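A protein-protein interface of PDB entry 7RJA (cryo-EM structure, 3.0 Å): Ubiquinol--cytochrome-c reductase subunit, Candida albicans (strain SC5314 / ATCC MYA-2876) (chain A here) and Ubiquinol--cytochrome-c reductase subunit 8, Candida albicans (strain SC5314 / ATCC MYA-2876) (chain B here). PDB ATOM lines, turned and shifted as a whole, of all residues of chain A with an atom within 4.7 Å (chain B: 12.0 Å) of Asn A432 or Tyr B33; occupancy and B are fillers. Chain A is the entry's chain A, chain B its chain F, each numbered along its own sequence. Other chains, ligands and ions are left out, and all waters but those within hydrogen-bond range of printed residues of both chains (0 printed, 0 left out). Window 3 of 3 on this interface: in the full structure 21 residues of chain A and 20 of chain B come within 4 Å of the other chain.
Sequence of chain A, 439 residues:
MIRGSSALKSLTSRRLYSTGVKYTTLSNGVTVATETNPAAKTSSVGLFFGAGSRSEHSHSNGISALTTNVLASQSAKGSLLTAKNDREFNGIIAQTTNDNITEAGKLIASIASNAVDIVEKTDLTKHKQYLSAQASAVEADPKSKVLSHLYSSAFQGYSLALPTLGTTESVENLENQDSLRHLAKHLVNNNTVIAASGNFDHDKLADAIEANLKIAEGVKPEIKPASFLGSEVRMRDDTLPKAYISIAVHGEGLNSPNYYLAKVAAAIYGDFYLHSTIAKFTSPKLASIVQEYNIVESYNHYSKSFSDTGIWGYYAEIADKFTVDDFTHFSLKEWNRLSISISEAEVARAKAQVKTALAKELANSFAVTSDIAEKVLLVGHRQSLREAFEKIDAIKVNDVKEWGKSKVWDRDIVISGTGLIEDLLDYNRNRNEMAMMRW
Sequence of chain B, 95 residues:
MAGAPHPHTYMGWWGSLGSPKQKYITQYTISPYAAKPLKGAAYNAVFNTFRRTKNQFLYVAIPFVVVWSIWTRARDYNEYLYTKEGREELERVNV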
ATOM      1  N   ASP A 412      14.599   4.527  24.291  1.00  0.00           N
ATOM      2  CA  ASP A 412      14.258   5.939  24.197  1.00  0.00           C
ATOM      3  C   ASP A 412      12.941   6.117  23.458  1.00  0.00           C
ATOM      4  O   ASP A 412      12.629   5.390  22.514  1.00  0.00           O
ATOM      5  CB  ASP A 412      15.356   6.717  23.477  1.00  0.00           C
ATOM      6  CG  ASP A 412      16.628   6.813  24.284  1.00  0.00           C
ATOM      7  OD1 ASP A 412      16.544   6.800  25.528  1.00  0.00           O
ATOM      8  OD2 ASP A 412      17.712   6.904  23.674  1.00  0.00           O
ATOM      9  N   ASN A 428      11.856  13.330  31.095  1.00  0.00           N
ATOM     10  CA  ASN A 428      12.418  12.358  32.027  1.00  0.00           C
ATOM     11  C   ASN A 428      11.347  11.523  32.710  1.00  0.00           C
ATOM     12  O   ASN A 428      11.547  10.323  32.909  1.00  0.00           O
ATOM     13  CB  ASN A 428      13.279  13.063  33.069  1.00  0.00           C
ATOM     14  CG  ASN A 428      14.550  13.611  32.484  1.00  0.00           C
ATOM     15  OD1 ASN A 428      14.781  14.816  32.483  1.00  0.00           O
ATOM     16  ND2 ASN A 428      15.393  12.723  31.981  1.00  0.00           N
ATOM     17  N   ARG A 429      10.209  12.114  33.064  1.00  0.00           N
ATOM     18  CA  ARG A 429       9.161  11.331  33.709  1.00  0.00           C
ATOM     19  C   ARG A 429       8.697  10.197  32.801  1.00  0.00           C
ATOM     20  O   ARG A 429       8.723   9.019  33.182  1.00  0.00           O
ATOM     21  CB  ARG A 429       7.995  12.245  34.086  1.00  0.00           C
ATOM     22  CG  ARG A 429       6.867  11.552  34.831  1.00  0.00           C
ATOM     23  CD  ARG A 429       7.303  11.064  36.202  1.00  0.00           C
ATOM     24  NE  ARG A 429       7.770  12.153  37.051  1.00  0.00           N
ATOM     25  CZ  ARG A 429       6.984  12.905  37.808  1.00  0.00           C
ATOM     26  NH1 ARG A 429       5.676  12.719  37.846  1.00  0.00           N
ATOM     27  NH2 ARG A 429       7.524  13.867  38.547  1.00  0.00           N
ATOM     28  N   ASN A 430       8.302  10.535  31.572  1.00  0.00           N
ATOM     29  CA  ASN A 430       7.802   9.518  30.654  1.00  0.00           C
ATOM     30  C   ASN A 430       8.884   8.506  30.312  1.00  0.00           C
ATOM     31  O   ASN A 430       8.619   7.302  30.241  1.00  0.00           O
ATOM     32  CB  ASN A 430       7.265  10.178  29.387  1.00  0.00           C
ATOM     33  CG  ASN A 430       6.213  11.223  29.679  1.00  0.00           C
ATOM     34  OD1 ASN A 430       6.287  12.348  29.193  1.00  0.00           O
ATOM     35  ND2 ASN A 430       5.223  10.856  30.481  1.00  0.00           N
ATOM     36  N   ARG A 431      10.113   8.973  30.097  1.00  0.00           N
ATOM     37  CA  ARG A 431      11.199   8.055  29.782  1.00  0.00           C
ATOM     38  C   ARG A 431      11.451   7.078  30.919  1.00  0.00           C
ATOM     39  O   ARG A 431      11.648   5.884  30.672  1.00  0.00           O
ATOM     40  CB  ARG A 431      12.469   8.840  29.461  1.00  0.00           C
ATOM     41  CG  ARG A 431      13.696   7.979  29.230  1.00  0.00           C
ATOM     42  CD  ARG A 431      13.511   7.054  28.049  1.00  0.00           C
ATOM     43  NE  ARG A 431      14.653   6.169  27.869  1.00  0.00           N
ATOM     44  CZ  ARG A 431      14.894   5.099  28.614  1.00  0.00           C
ATOM     45  NH1 ARG A 431      14.109   4.771  29.626  1.00  0.00           N
ATOM     46  NH2 ARG A 431      15.950   4.342  28.338  1.00  0.00           N
ATOM     47  N   ASN A 432      11.443   7.553  32.164  1.00  0.00           N
ATOM     48  CA  ASN A 432      11.659   6.660  33.292  1.00  0.00           C
ATOM     49  C   ASN A 432      10.490   5.709  33.475  1.00  0.00           C
ATOM     50  O   ASN A 432      10.663   4.619  34.029  1.00  0.00           O
ATOM     51  CB  ASN A 432      11.888   7.469  34.564  1.00  0.00           C
ATOM     52  CG  ASN A 432      13.257   8.109  34.602  1.00  0.00           C
ATOM     53  OD1 ASN A 432      14.242   7.520  34.158  1.00  0.00           O
ATOM     54  ND2 ASN A 432      13.328   9.324  35.132  1.00  0.00           N
ATOM     55  N   GLU A 433       9.298   6.092  33.015  1.00  0.00           N
ATOM     56  CA  GLU A 433       8.182   5.154  33.070  1.00  0.00           C
ATOM     57  C   GLU A 433       8.416   3.912  32.221  1.00  0.00           C
ATOM     58  O   GLU A 433       7.694   2.926  32.395  1.00  0.00           O
ATOM     59  CB  GLU A 433       6.882   5.825  32.625  1.00  0.00           C
ATOM     60  CG  GLU A 433       6.388   6.922  33.548  1.00  0.00           C
ATOM     61  CD  GLU A 433       5.962   6.396  34.901  1.00  0.00           C
ATOM     62  OE1 GLU A 433       5.478   5.247  34.967  1.00  0.00           O
ATOM     63  OE2 GLU A 433       6.109   7.131  35.901  1.00  0.00           O
ATOM     64  N   MET A 434       9.396   3.931  31.319  1.00  0.00           N
ATOM     65  CA  MET A 434       9.617   2.820  30.400  1.00  0.00           C
ATOM     66  C   MET A 434      10.312   1.624  31.037  1.00  0.00           C
ATOM     67  O   MET A 434      10.474   0.605  30.361  1.00  0.00           O
ATOM     68  CB  MET A 434      10.451   3.283  29.206  1.00  0.00           C
ATOM     69  CG  MET A 434       9.791   4.342  28.353  1.00  0.00           C
ATOM     70  SD  MET A 434       8.389   3.690  27.442  1.00  0.00           S
ATOM     71  CE  MET A 434       9.230   2.809  26.136  1.00  0.00           C
ATOM     72  N   ALA A 435      10.740   1.715  32.300  1.00  0.00           N
ATOM     73  CA  ALA A 435      11.523   0.635  32.890  1.00  0.00           C
ATOM     74  C   ALA A 435      11.158   0.318  34.335  1.00  0.00           C
ATOM     75  O   ALA A 435      11.846  -0.500  34.959  1.00  0.00           O
ATOM     76  CB  ALA A 435      13.013   0.970  32.812  1.00  0.00           C
ATOM     77  N   MET A 436      10.114   0.922  34.893  1.00  0.00           N
ATOM     78  CA  MET A 436       9.748   0.683  36.289  1.00  0.00           C
ATOM     79  C   MET A 436       8.884  -0.569  36.356  1.00  0.00           C
ATOM     80  O   MET A 436       7.657  -0.511  36.255  1.00  0.00           O
ATOM     81  CB  MET A 436       9.034   1.892  36.877  1.00  0.00           C
ATOM     82  CG  MET A 436       9.962   2.882  37.560  1.00  0.00           C
ATOM     83  SD  MET A 436       9.080   4.072  38.591  1.00  0.00           S
ATOM     84  CE  MET A 436      10.412   5.185  39.031  1.00  0.00           C
ATOM     85  N   THR B  29      13.648  19.153  22.607  1.00  0.00           N
ATOM     86  CA  THR B  29      14.668  18.629  23.504  1.00  0.00           C
ATOM     87  C   THR B  29      15.029  17.224  23.054  1.00  0.00           C
ATOM     88  O   THR B  29      14.281  16.574  22.322  1.00  0.00           O
ATOM     89  CB  THR B  29      14.196  18.628  24.958  1.00  0.00           C
ATOM     90  OG1 THR B  29      15.251  18.153  25.801  1.00  0.00           O
ATOM     91  CG2 THR B  29      12.990  17.742  25.127  1.00  0.00           C
ATOM     92  N   ILE B  30      16.190  16.764  23.502  1.00  0.00           N
ATOM     93  CA  ILE B  30      16.666  15.429  23.194  1.00  0.00           C
ATOM     94  C   ILE B  30      16.659  14.608  24.475  1.00  0.00           C
ATOM     95  O   ILE B  30      16.710  15.138  25.583  1.00  0.00           O
ATOM     96  CB  ILE B  30      18.065  15.444  22.554  1.00  0.00           C
ATOM     97  CG1 ILE B  30      19.068  16.136  23.479  1.00  0.00           C
ATOM     98  CG2 ILE B  30      18.017  16.139  21.212  1.00  0.00           C
ATOM     99  CD1 ILE B  30      20.477  16.155  22.939  1.00  0.00           C
ATOM    100  N   SER B  31      16.609  13.384  24.322  1.00  0.00           N
ATOM    101  CA  SER B  31      16.576  12.512  25.477  1.00  0.00           C
ATOM    102  C   SER B  31      17.935  12.470  26.156  1.00  0.00           C
ATOM    103  O   SER B  31      18.957  12.759  25.531  1.00  0.00           O
ATOM    104  CB  SER B  31      16.194  11.099  25.062  1.00  0.00           C
ATOM    105  OG  SER B  31      17.328  10.395  24.595  1.00  0.00           O
ATOM    106  N   PRO B  32      17.981  12.113  27.434  1.00  0.00           N
ATOM    107  CA  PRO B  32      19.227  11.590  27.983  1.00  0.00           C
ATOM    108  C   PRO B  32      19.452  10.202  27.414  1.00  0.00           C
ATOM    109  O   PRO B  32      18.576   9.632  26.762  1.00  0.00           O
ATOM    110  CB  PRO B  32      18.971  11.565  29.488  1.00  0.00           C
ATOM    111  CG  PRO B  32      17.513  11.381  29.611  1.00  0.00           C
ATOM    112  CD  PRO B  32      16.860  11.940  28.372  1.00  0.00           C
ATOM    113  N   TYR B  33      20.650   9.669  27.634  1.00  0.00           N
ATOM    114  CA  TYR B  33      21.070   8.441  26.970  1.00  0.00           C
ATOM    115  C   TYR B  33      21.391   8.722  25.508  1.00  0.00           C
ATOM    116  O   TYR B  33      21.851   7.830  24.788  1.00  0.00           O
ATOM    117  CB  TYR B  33      19.999   7.347  27.049  1.00  0.00           C
ATOM    118  CG  TYR B  33      19.332   7.183  28.395  1.00  0.00           C
ATOM    119  CD1 TYR B  33      20.048   6.757  29.499  1.00  0.00           C
ATOM    120  CD2 TYR B  33      17.981   7.433  28.553  1.00  0.00           C
ATOM    121  CE1 TYR B  33      19.438   6.595  30.723  1.00  0.00           C
ATOM    122  CE2 TYR B  33      17.365   7.278  29.773  1.00  0.00           C
ATOM    123  CZ  TYR B  33      18.098   6.860  30.854  1.00  0.00           C
ATOM    124  OH  TYR B  33      17.483   6.704  32.073  1.00  0.00           O
ATOM    125  N   ALA B  34      21.148   9.954  25.056  1.00  0.00           N
ATOM    126  CA  ALA B  34      21.398  10.355  23.678  1.00  0.00           C
ATOM    127  C   ALA B  34      22.001  11.749  23.633  1.00  0.00           C
ATOM    128  O   ALA B  34      22.044  12.381  22.576  1.00  0.00           O
ATOM    129  CB  ALA B  34      20.118  10.301  22.849  1.00  0.00           C
ATOM    130  N   ALA B  35      22.455  12.244  24.778  1.00  0.00           N
ATOM    131  CA  ALA B  35      23.119  13.532  24.875  1.00  0.00           C
ATOM    132  C   ALA B  35      24.403  13.357  25.666  1.00  0.00           C
ATOM    133  O   ALA B  35      24.489  12.503  26.550  1.00  0.00           O
ATOM    134  CB  ALA B  35      22.225  14.577  25.549  1.00  0.00           C
ATOM    135  N   LYS B  36      25.402  14.172  25.343  1.00  0.00           N
ATOM    136  CA  LYS B  36      26.679  14.102  26.037  1.00  0.00           C
ATOM    137  C   LYS B  36      26.532  14.686  27.436  1.00  0.00           C
ATOM    138  O   LYS B  36      26.485  15.914  27.582  1.00  0.00           O
ATOM    139  CB  LYS B  36      27.759  14.865  25.269  1.00  0.00           C
ATOM    140  CG  LYS B  36      28.151  14.250  23.940  1.00  0.00           C
ATOM    141  CD  LYS B  36      29.248  15.069  23.277  1.00  0.00           C
ATOM    142  CE  LYS B  36      29.649  14.493  21.932  1.00  0.00           C
ATOM    143  NZ  LYS B  36      30.714  15.304  21.284  1.00  0.00           N
ATOM    144  N   PRO B  37      26.462  13.870  28.485  1.00  0.00           N
ATOM    145  CA  PRO B  37      26.364  14.436  29.831  1.00  0.00           C
ATOM    146  C   PRO B  37      27.644  15.165  30.189  1.00  0.00           C
ATOM    147  O   PRO B  37      28.742  14.788  29.771  1.00  0.00           O
ATOM    148  CB  PRO B  37      26.146  13.206  30.726  1.00  0.00           C
ATOM    149  CG  PRO B  37      25.949  12.043  29.785  1.00  0.00           C
ATOM    150  CD  PRO B  37      26.687  12.418  28.548  1.00  0.00           C
ATOM    151  N   LEU B  38      27.495  16.228  30.972  1.00  0.00           N
ATOM    152  CA  LEU B  38      28.620  17.094  31.302  1.00  0.00           C
ATOM    153  C   LEU B  38      29.306  17.563  30.021  1.00  0.00           C
ATOM    154  O   LEU B  38      30.532  17.552  29.896  1.00  0.00           O
ATOM    155  CB  LEU B  38      29.609  16.375  32.223  1.00  0.00           C
ATOM    156  CG  LEU B  38      29.101  16.037  33.627  1.00  0.00           C
ATOM    157  CD1 LEU B  38      28.207  14.808  33.601  1.00  0.00           C
ATOM    158  CD2 LEU B  38      30.264  15.826  34.582  1.00  0.00           C
ATOM    159  N   LYS B  39      28.483  17.975  29.052  1.00  0.00           N
ATOM    160  CA  LYS B  39      28.991  18.288  27.719  1.00  0.00           C
ATOM    161  C   LYS B  39      30.144  19.281  27.789  1.00  0.00           C
ATOM    162  O   LYS B  39      31.201  19.067  27.186  1.00  0.00           O
ATOM    163  CB  LYS B  39      27.856  18.832  26.849  1.00  0.00           C
ATOM    164  CG  LYS B  39      28.294  19.435  25.516  1.00  0.00           C
ATOM    165  CD  LYS B  39      28.808  18.366  24.566  1.00  0.00           C
ATOM    166  CE  LYS B  39      29.379  18.971  23.294  1.00  0.00           C
ATOM    167  NZ  LYS B  39      30.583  19.807  23.554  1.00  0.00           N
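Of the printed residues of chain B, Asp A412 touches Ser B31, Pro B32 and Tyr B33.
No residue of chain B comes within 4 Å of Asn A430.
Arg A431 touches just one residue of chain B: Tyr B33 (3.5 Å).
Asn A432 touches one residue of chain B.
No residue of chain B comes within 4 Å of Glu A433.
No residue of chain B comes within 4 Å of Ala A435.
Printed residues of chain A within 4 Å of Ser B31: Asp A412.
Printed residues of chain A within 4 Å of Pro B32: Asp A412 (3.7 Å) and Asn A428 (3.5 Å).
Of chain A, only Asp A412, Arg A431 and Asn A432 come within 4 Å of Tyr B33.
The nearest printed residue of chain A that does not touch Pro B32 is Arg A431 (5.1 Å).
Printed residues of chain A that touch a printed residue of chain B: Asp A412, Asn A428, Arg A431 and Asn A432.
Among the printed residues, no Asp or Glu carboxylate lies within 4 Å of a Lys or Arg side-chain nitrogen of the other chain.
Asp A412 touches Ser B31 (OD2 to OG, 3.6 Å).
OD1 of Asp A412 touches O of Pro B32, 3.7 Å away.
CD2 of Tyr B33 touches OD1 of Asp A412, 3.4 Å away.
Asn A428 touches Pro B32 (ND2 to CG, 3.5 Å).
Tyr B33 touches Arg A431.
Tyr B33 touches Asn A432.
ND2 of Asn A432 sits at hydrogen-bond distance from O of Asn A428, 3.0 Å away.
The side-chain carboxylate (OD1) of Asp A412 lies within salt-bridge range of the guanidinium group (NE) of Arg A431, 3.1 Å away.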
